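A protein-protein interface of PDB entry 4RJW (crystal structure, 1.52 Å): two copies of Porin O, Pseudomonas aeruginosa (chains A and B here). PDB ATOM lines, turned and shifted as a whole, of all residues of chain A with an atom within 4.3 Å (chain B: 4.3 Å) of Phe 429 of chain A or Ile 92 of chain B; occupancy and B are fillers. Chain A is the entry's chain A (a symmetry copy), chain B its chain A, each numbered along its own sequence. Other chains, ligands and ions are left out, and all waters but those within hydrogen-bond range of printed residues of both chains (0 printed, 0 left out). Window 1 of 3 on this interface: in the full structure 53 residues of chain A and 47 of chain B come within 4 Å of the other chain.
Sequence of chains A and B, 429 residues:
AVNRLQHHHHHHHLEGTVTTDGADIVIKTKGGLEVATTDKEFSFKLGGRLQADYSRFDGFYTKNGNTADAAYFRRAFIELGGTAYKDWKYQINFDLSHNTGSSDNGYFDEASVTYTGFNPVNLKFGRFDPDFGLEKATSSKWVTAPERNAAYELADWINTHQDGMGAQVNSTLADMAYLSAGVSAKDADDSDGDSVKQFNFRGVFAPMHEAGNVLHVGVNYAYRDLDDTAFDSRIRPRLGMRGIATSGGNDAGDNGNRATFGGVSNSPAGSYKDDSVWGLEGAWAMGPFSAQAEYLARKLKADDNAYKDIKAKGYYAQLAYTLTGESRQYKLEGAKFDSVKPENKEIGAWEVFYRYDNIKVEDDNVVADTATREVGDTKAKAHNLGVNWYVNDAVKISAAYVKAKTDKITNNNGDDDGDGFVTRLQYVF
N of Gly 32 of chain A is in hydrogen-bond range of OXT of Phe 429 of chain A (3.4 Å). The backbone NH of Gly 48 of chain A sits at hydrogen-bond distance from the chain-end carboxylate of Phe 429 of chain A. The backbone NH (N) of Ile 92 of chain B lies within hydrogen-bond range of the backbone carbonyl oxygen (O) of Leu 80 of chain B (2.7 Å). The backbone NH of Ile 78 of chain B lies within hydrogen-bond range of the backbone carbonyl oxygen of Phe 94 of chain B, 2.9 Å away. The backbone NH (N) of Leu 50 of chain A sits at hydrogen-bond distance from the backbone carbonyl oxygen (O) of Tyr 427 of chain A (2.9 Å).
The side-chain hydroxyl of Tyr 90 of chain B lies within hydrogen-bond range of the backbone carbonyl oxygen of Gly 31 of chain A (2.7 Å).
Of the printed residues of chain B, Gly 31 of chain A touches Tyr 90. Arg 49 of chain A touches none of the printed residues of chain B. Of the printed residues of chain B, Leu 50 of chain A touches Ile 92 (3.5 Å). Printed residues of chain B within 4 Å of Leu 96 of chain A: Ile 92 (3.6 Å) and Phe 94 (3.6 Å). Printed residues of chain B within 4 Å of Tyr 427 of chain A: Tyr 90. Phe 429 of chain A touches two residues of chain B. Printed residues of chain A within 4 Å of Tyr 90 of chain B: Gly 31 (2.7 Å), Tyr 427 (3.4 Å) and Phe 429 (3.1 Å). Printed residues of chain A within 4 Å of Ile 92 of chain B: Leu 50 (3.5 Å), Leu 96 (3.6 Å) and Phe 429 (3.8 Å). Asn 93 of chain B touches none of the printed residues of chain A.
Among the printed residues, pairs that only touch across the chains: Leu 50 of chain A with Ile 92 of chain B (3.5 Å), Leu 96 of chain A with Ile 92 of chain B (3.6 Å), Leu 96 of chain A with Phe 94 of chain B (3.6 Å), Tyr 427 of chain A with Tyr 90 of chain B (3.4 Å), Phe 429 of chain A with Tyr 90 of chain B (3.1 Å) and Phe 429 of chain A with Ile 92 of chain B (3.8 Å).
Of the 9 printed residues of chain B, 3 touch a printed residue of chain A. Along chain B the printed residues that touch a printed residue of chain A span positions 90 to 94. Hydrophobic or aromatic side chains of chain A within 4 Å of the printed part of chain B: Leu 50, Leu 96, Tyr 427 and Phe 429. Among the printed residues, 7 pairs touch across the chains. Among the printed residues, no Asp or Glu carboxylate lies within 4 Å of a Lys or Arg side-chain nitrogen of the other chain.
No position is printed for both chains. Of the 7 pairs that touch across the chains among the printed residues, none has its exchanged pair printed and touching as well.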
ATOM      1  N   GLY A  31      14.535  20.378 -21.369  1.00  0.00           N
ATOM      2  CA  GLY A  31      13.889  21.639 -21.699  1.00  0.00           C
ATOM      3  C   GLY A  31      14.210  22.742 -20.705  1.00  0.00           C
ATOM      4  O   GLY A  31      14.072  23.919 -21.016  1.00  0.00           O
ATOM      5  N   GLY A  32      14.613  22.355 -19.500  1.00  0.00           N
ATOM      6  CA  GLY A  32      15.120  23.277 -18.492  1.00  0.00           C
ATOM      7  C   GLY A  32      16.548  22.910 -18.147  1.00  0.00           C
ATOM      8  O   GLY A  32      17.314  22.500 -19.012  1.00  0.00           O
ATOM      9  N   LEU A  46      16.406  24.607 -12.662  1.00  0.00           N
ATOM     10  CA  LEU A  46      15.587  25.674 -13.208  1.00  0.00           C
ATOM     11  C   LEU A  46      14.541  25.037 -14.108  1.00  0.00           C
ATOM     12  O   LEU A  46      14.872  24.301 -15.051  1.00  0.00           O
ATOM     13  CB  LEU A  46      16.455  26.672 -13.978  1.00  0.00           C
ATOM     14  CG  LEU A  46      15.773  27.860 -14.659  1.00  0.00           C
ATOM     15  CD1 LEU A  46      14.926  28.632 -13.667  1.00  0.00           C
ATOM     16  CD2 LEU A  46      16.828  28.768 -15.244  1.00  0.00           C
ATOM     17  N   GLY A  47      13.271  25.284 -13.795  1.00  0.00           N
ATOM     18  CA  GLY A  47      12.171  24.732 -14.567  1.00  0.00           C
ATOM     19  C   GLY A  47      10.998  25.677 -14.584  1.00  0.00           C
ATOM     20  O   GLY A  47      11.145  26.874 -14.339  1.00  0.00           O
ATOM     21  N   GLY A  48       9.824  25.138 -14.870  1.00  0.00           N
ATOM     22  CA  GLY A  48       8.640  25.969 -14.903  1.00  0.00           C
ATOM     23  C   GLY A  48       7.467  25.231 -15.495  1.00  0.00           C
ATOM     24  O   GLY A  48       7.541  24.047 -15.832  1.00  0.00           O
ATOM     25  N   ARG A  49       6.364  25.953 -15.624  1.00  0.00           N
ATOM     26  CA  ARG A  49       5.171  25.371 -16.205  1.00  0.00           C
ATOM     27  C   ARG A  49       4.338  26.471 -16.833  1.00  0.00           C
ATOM     28  O   ARG A  49       4.142  27.543 -16.250  1.00  0.00           O
ATOM     29  CB  ARG A  49       4.372  24.582 -15.146  1.00  0.00           C
ATOM     30  CG  ARG A  49       3.608  25.439 -14.123  1.00  0.00           C
ATOM     31  CD  ARG A  49       3.169  24.577 -12.942  1.00  0.00           C
ATOM     32  NE  ARG A  49       4.321  24.159 -12.144  1.00  0.00           N
ATOM     33  CZ  ARG A  49       4.236  23.545 -10.970  1.00  0.00           C
ATOM     34  NH1 ARG A  49       5.342  23.229 -10.307  1.00  0.00           N
ATOM     35  NH2 ARG A  49       3.045  23.236 -10.470  1.00  0.00           N
ATOM     36  N   LEU A  50       3.894  26.209 -18.052  1.00  0.00           N
ATOM     37  CA  LEU A  50       2.995  27.113 -18.761  1.00  0.00           C
ATOM     38  C   LEU A  50       1.674  26.405 -18.944  1.00  0.00           C
ATOM     39  O   LEU A  50       1.636  25.291 -19.440  1.00  0.00           O
ATOM     40  CB  LEU A  50       3.545  27.435 -20.144  1.00  0.00           C
ATOM     41  CG  LEU A  50       4.769  28.326 -20.277  1.00  0.00           C
ATOM     42  CD1 LEU A  50       5.093  28.536 -21.748  1.00  0.00           C
ATOM     43  CD2 LEU A  50       4.523  29.658 -19.587  1.00  0.00           C
ATOM     44  N   LEU A  96       4.429  34.276 -13.335  1.00  0.00           N
ATOM     45  CA  LEU A  96       4.424  35.408 -14.260  1.00  0.00           C
ATOM     46  C   LEU A  96       3.019  35.806 -14.711  1.00  0.00           C
ATOM     47  O   LEU A  96       2.825  36.938 -15.135  1.00  0.00           O
ATOM     48  CB  LEU A  96       5.273  35.100 -15.487  1.00  0.00           C
ATOM     49  CG  LEU A  96       6.750  34.845 -15.217  1.00  0.00           C
ATOM     50  CD1 LEU A  96       7.373  34.373 -16.517  1.00  0.00           C
ATOM     51  CD2 LEU A  96       7.422  36.114 -14.709  1.00  0.00           C
ATOM     52  N   TYR A 427       2.859  23.132 -20.977  1.00  0.00           N
ATOM     53  CA  TYR A 427       4.241  22.781 -21.240  1.00  0.00           C
ATOM     54  C   TYR A 427       5.001  22.838 -19.923  1.00  0.00           C
ATOM     55  O   TYR A 427       5.040  23.875 -19.255  1.00  0.00           O
ATOM     56  CB  TYR A 427       4.837  23.769 -22.255  1.00  0.00           C
ATOM     57  CG  TYR A 427       6.133  23.326 -22.928  1.00  0.00           C
ATOM     58  CD1 TYR A 427       7.267  23.022 -22.184  1.00  0.00           C
ATOM     59  CD2 TYR A 427       6.222  23.250 -24.313  1.00  0.00           C
ATOM     60  CE1 TYR A 427       8.452  22.629 -22.805  1.00  0.00           C
ATOM     61  CE2 TYR A 427       7.402  22.872 -24.940  1.00  0.00           C
ATOM     62  CZ  TYR A 427       8.511  22.558 -24.183  1.00  0.00           C
ATOM     63  OH  TYR A 427       9.680  22.176 -24.815  1.00  0.00           O
ATOM     64  N   VAL A 428       5.611  21.719 -19.549  1.00  0.00           N
ATOM     65  CA  VAL A 428       6.397  21.638 -18.328  1.00  0.00           C
ATOM     66  C   VAL A 428       7.862  21.482 -18.713  1.00  0.00           C
ATOM     67  O   VAL A 428       8.197  20.685 -19.587  1.00  0.00           O
ATOM     68  CB  VAL A 428       5.948  20.419 -17.485  1.00  0.00           C
ATOM     69  CG1 VAL A 428       6.950  20.117 -16.369  1.00  0.00           C
ATOM     70  CG2 VAL A 428       4.523  20.644 -16.949  1.00  0.00           C
ATOM     71  N   PHE A 429       8.735  22.272 -18.094  1.00  0.00           N
ATOM     72  CA  PHE A 429      10.162  22.189 -18.379  1.00  0.00           C
ATOM     73  C   PHE A 429      10.993  22.235 -17.105  1.00  0.00           C
ATOM     74  O   PHE A 429      10.473  22.487 -16.019  1.00  0.00           O
ATOM     75  CB  PHE A 429      10.602  23.300 -19.352  1.00  0.00           C
ATOM     76  CG  PHE A 429      10.315  24.691 -18.866  1.00  0.00           C
ATOM     77  CD1 PHE A 429       9.077  25.280 -19.094  1.00  0.00           C
ATOM     78  CD2 PHE A 429      11.291  25.426 -18.200  1.00  0.00           C
ATOM     79  CE1 PHE A 429       8.815  26.567 -18.653  1.00  0.00           C
ATOM     80  CE2 PHE A 429      11.036  26.707 -17.765  1.00  0.00           C
ATOM     81  CZ  PHE A 429       9.800  27.284 -17.989  1.00  0.00           C
ATOM     82  OXT PHE A 429      12.209  22.010 -17.164  1.00  0.00           O
ATOM     83  N   ILE B  78      14.136  39.030 -19.251  1.00  0.00           N
ATOM     84  CA  ILE B  78      14.731  37.738 -18.963  1.00  0.00           C
ATOM     85  C   ILE B  78      14.053  36.751 -19.908  1.00  0.00           C
ATOM     86  O   ILE B  78      12.824  36.762 -20.043  1.00  0.00           O
ATOM     87  CB  ILE B  78      14.469  37.325 -17.512  1.00  0.00           C
ATOM     88  CG1 ILE B  78      14.977  38.401 -16.536  1.00  0.00           C
ATOM     89  CG2 ILE B  78      15.116  35.951 -17.241  1.00  0.00           C
ATOM     90  CD1 ILE B  78      16.449  38.789 -16.753  1.00  0.00           C
ATOM     91  N   GLU B  79      14.855  35.909 -20.561  1.00  0.00           N
ATOM     92  CA  GLU B  79      14.380  35.067 -21.653  1.00  0.00           C
ATOM     93  C   GLU B  79      14.704  33.600 -21.395  1.00  0.00           C
ATOM     94  O   GLU B  79      15.877  33.222 -21.287  1.00  0.00           O
ATOM     95  CB  GLU B  79      15.011  35.540 -22.971  1.00  0.00           C
ATOM     96  CG  GLU B  79      14.653  36.987 -23.290  1.00  0.00           C
ATOM     97  CD  GLU B  79      15.519  37.628 -24.353  1.00  0.00           C
ATOM     98  OE1 GLU B  79      16.048  36.912 -25.230  1.00  0.00           O
ATOM     99  OE2 GLU B  79      15.679  38.866 -24.295  1.00  0.00           O
ATOM    100  N   LEU B  80      13.668  32.780 -21.263  1.00  0.00           N
ATOM    101  CA  LEU B  80      13.859  31.333 -21.113  1.00  0.00           C
ATOM    102  C   LEU B  80      13.206  30.635 -22.280  1.00  0.00           C
ATOM    103  O   LEU B  80      12.024  30.848 -22.545  1.00  0.00           O
ATOM    104  CB  LEU B  80      13.212  30.820 -19.822  1.00  0.00           C
ATOM    105  CG  LEU B  80      13.890  31.084 -18.480  1.00  0.00           C
ATOM    106  CD1 LEU B  80      13.582  32.476 -17.981  1.00  0.00           C
ATOM    107  CD2 LEU B  80      13.432  30.033 -17.462  1.00  0.00           C
ATOM    108  N   TYR B  90       9.378  26.111 -26.432  1.00  0.00           N
ATOM    109  CA  TYR B  90       8.707  27.170 -25.686  1.00  0.00           C
ATOM    110  C   TYR B  90       9.623  28.365 -25.627  1.00  0.00           C
ATOM    111  O   TYR B  90      10.845  28.240 -25.775  1.00  0.00           O
ATOM    112  CB  TYR B  90       8.330  26.720 -24.267  1.00  0.00           C
ATOM    113  CG  TYR B  90       9.509  26.618 -23.323  1.00  0.00           C
ATOM    114  CD1 TYR B  90      10.286  25.471 -23.280  1.00  0.00           C
ATOM    115  CD2 TYR B  90       9.859  27.679 -22.488  1.00  0.00           C
ATOM    116  CE1 TYR B  90      11.373  25.368 -22.431  1.00  0.00           C
ATOM    117  CE2 TYR B  90      10.959  27.591 -21.640  1.00  0.00           C
ATOM    118  CZ  TYR B  90      11.707  26.437 -21.617  1.00  0.00           C
ATOM    119  OH  TYR B  90      12.797  26.325 -20.788  1.00  0.00           O
ATOM    120  N   GLN B  91       9.028  29.531 -25.420  1.00  0.00           N
ATOM    121  CA  GLN B  91       9.800  30.745 -25.222  1.00  0.00           C
ATOM    122  C   GLN B  91       9.025  31.646 -24.293  1.00  0.00           C
ATOM    123  O   GLN B  91       7.869  31.982 -24.566  1.00  0.00           O
ATOM    124  CB  GLN B  91      10.042  31.464 -26.548  1.00  0.00           C
ATOM    125  CG  GLN B  91      11.005  32.632 -26.435  1.00  0.00           C
ATOM    126  CD  GLN B  91      12.406  32.179 -26.108  1.00  0.00           C
ATOM    127  OE1 GLN B  91      12.902  31.203 -26.671  1.00  0.00           O
ATOM    128  NE2 GLN B  91      13.054  32.881 -25.180  1.00  0.00           N
ATOM    129  N   ILE B  92       9.658  32.026 -23.189  1.00  0.00           N
ATOM    130  CA  ILE B  92       9.045  32.920 -22.209  1.00  0.00           C
ATOM    131  C   ILE B  92       9.985  34.085 -21.972  1.00  0.00           C
ATOM    132  O   ILE B  92      11.076  33.922 -21.405  1.00  0.00           O
ATOM    133  CB  ILE B  92       8.800  32.211 -20.869  1.00  0.00           C
ATOM    134  CG1 ILE B  92       7.904  30.994 -21.063  1.00  0.00           C
ATOM    135  CG2 ILE B  92       8.178  33.165 -19.853  1.00  0.00           C
ATOM    136  CD1 ILE B  92       7.986  30.010 -19.893  1.00  0.00           C
ATOM    137  N   ASN B  93       9.559  35.261 -22.417  1.00  0.00           N
ATOM    138  CA  ASN B  93      10.330  36.476 -22.243  1.00  0.00           C
ATOM    139  C   ASN B  93       9.521  37.400 -21.379  1.00  0.00           C
ATOM    140  O   ASN B  93       8.437  37.839 -21.777  1.00  0.00           O
ATOM    141  CB  ASN B  93      10.587  37.164 -23.585  1.00  0.00           C
ATOM    142  CG  ASN B  93      11.378  36.303 -24.542  1.00  0.00           C
ATOM    143  OD1 ASN B  93      12.032  35.335 -24.146  1.00  0.00           O
ATOM    144  ND2 ASN B  93      11.336  36.673 -25.817  1.00  0.00           N
ATOM    145  N   PHE B  94      10.037  37.701 -20.195  1.00  0.00           N
ATOM    146  CA  PHE B  94       9.330  38.617 -19.308  1.00  0.00           C
ATOM    147  C   PHE B  94      10.123  39.896 -19.111  1.00  0.00           C
ATOM    148  O   PHE B  94      11.349  39.856 -18.996  1.00  0.00           O
ATOM    149  CB  PHE B  94       8.893  37.952 -17.985  1.00  0.00           C
ATOM    150  CG  PHE B  94      10.002  37.323 -17.161  1.00  0.00           C
ATOM    151  CD1 PHE B  94      10.450  36.036 -17.430  1.00  0.00           C
ATOM    152  CD2 PHE B  94      10.506  37.979 -16.045  1.00  0.00           C
ATOM    153  CE1 PHE B  94      11.417  35.432 -16.631  1.00  0.00           C
ATOM    154  CE2 PHE B  94      11.476  37.386 -15.240  1.00  0.00           C
ATOM    155  CZ  PHE B  94      11.929  36.116 -15.533  1.00  0.00           C
ATOM    156  N   GLU B 110       6.710  37.718 -24.605  1.00  0.00           N
ATOM    157  CA  GLU B 110       6.288  36.497 -25.283  1.00  0.00           C
ATOM    158  C   GLU B 110       6.097  35.390 -24.252  1.00  0.00           C
ATOM    159  O   GLU B 110       6.880  35.271 -23.311  1.00  0.00           O
ATOM    160  CB  GLU B 110       7.357  36.055 -26.298  1.00  0.00           C
ATOM    161  CG  GLU B 110       6.963  34.814 -27.079  1.00  0.00           C
ATOM    162  CD  GLU B 110       7.966  34.451 -28.159  1.00  0.00           C
ATOM    163  OE1 GLU B 110       8.981  35.173 -28.328  1.00  0.00           O
ATOM    164  OE2 GLU B 110       7.737  33.438 -28.843  1.00  0.00           O
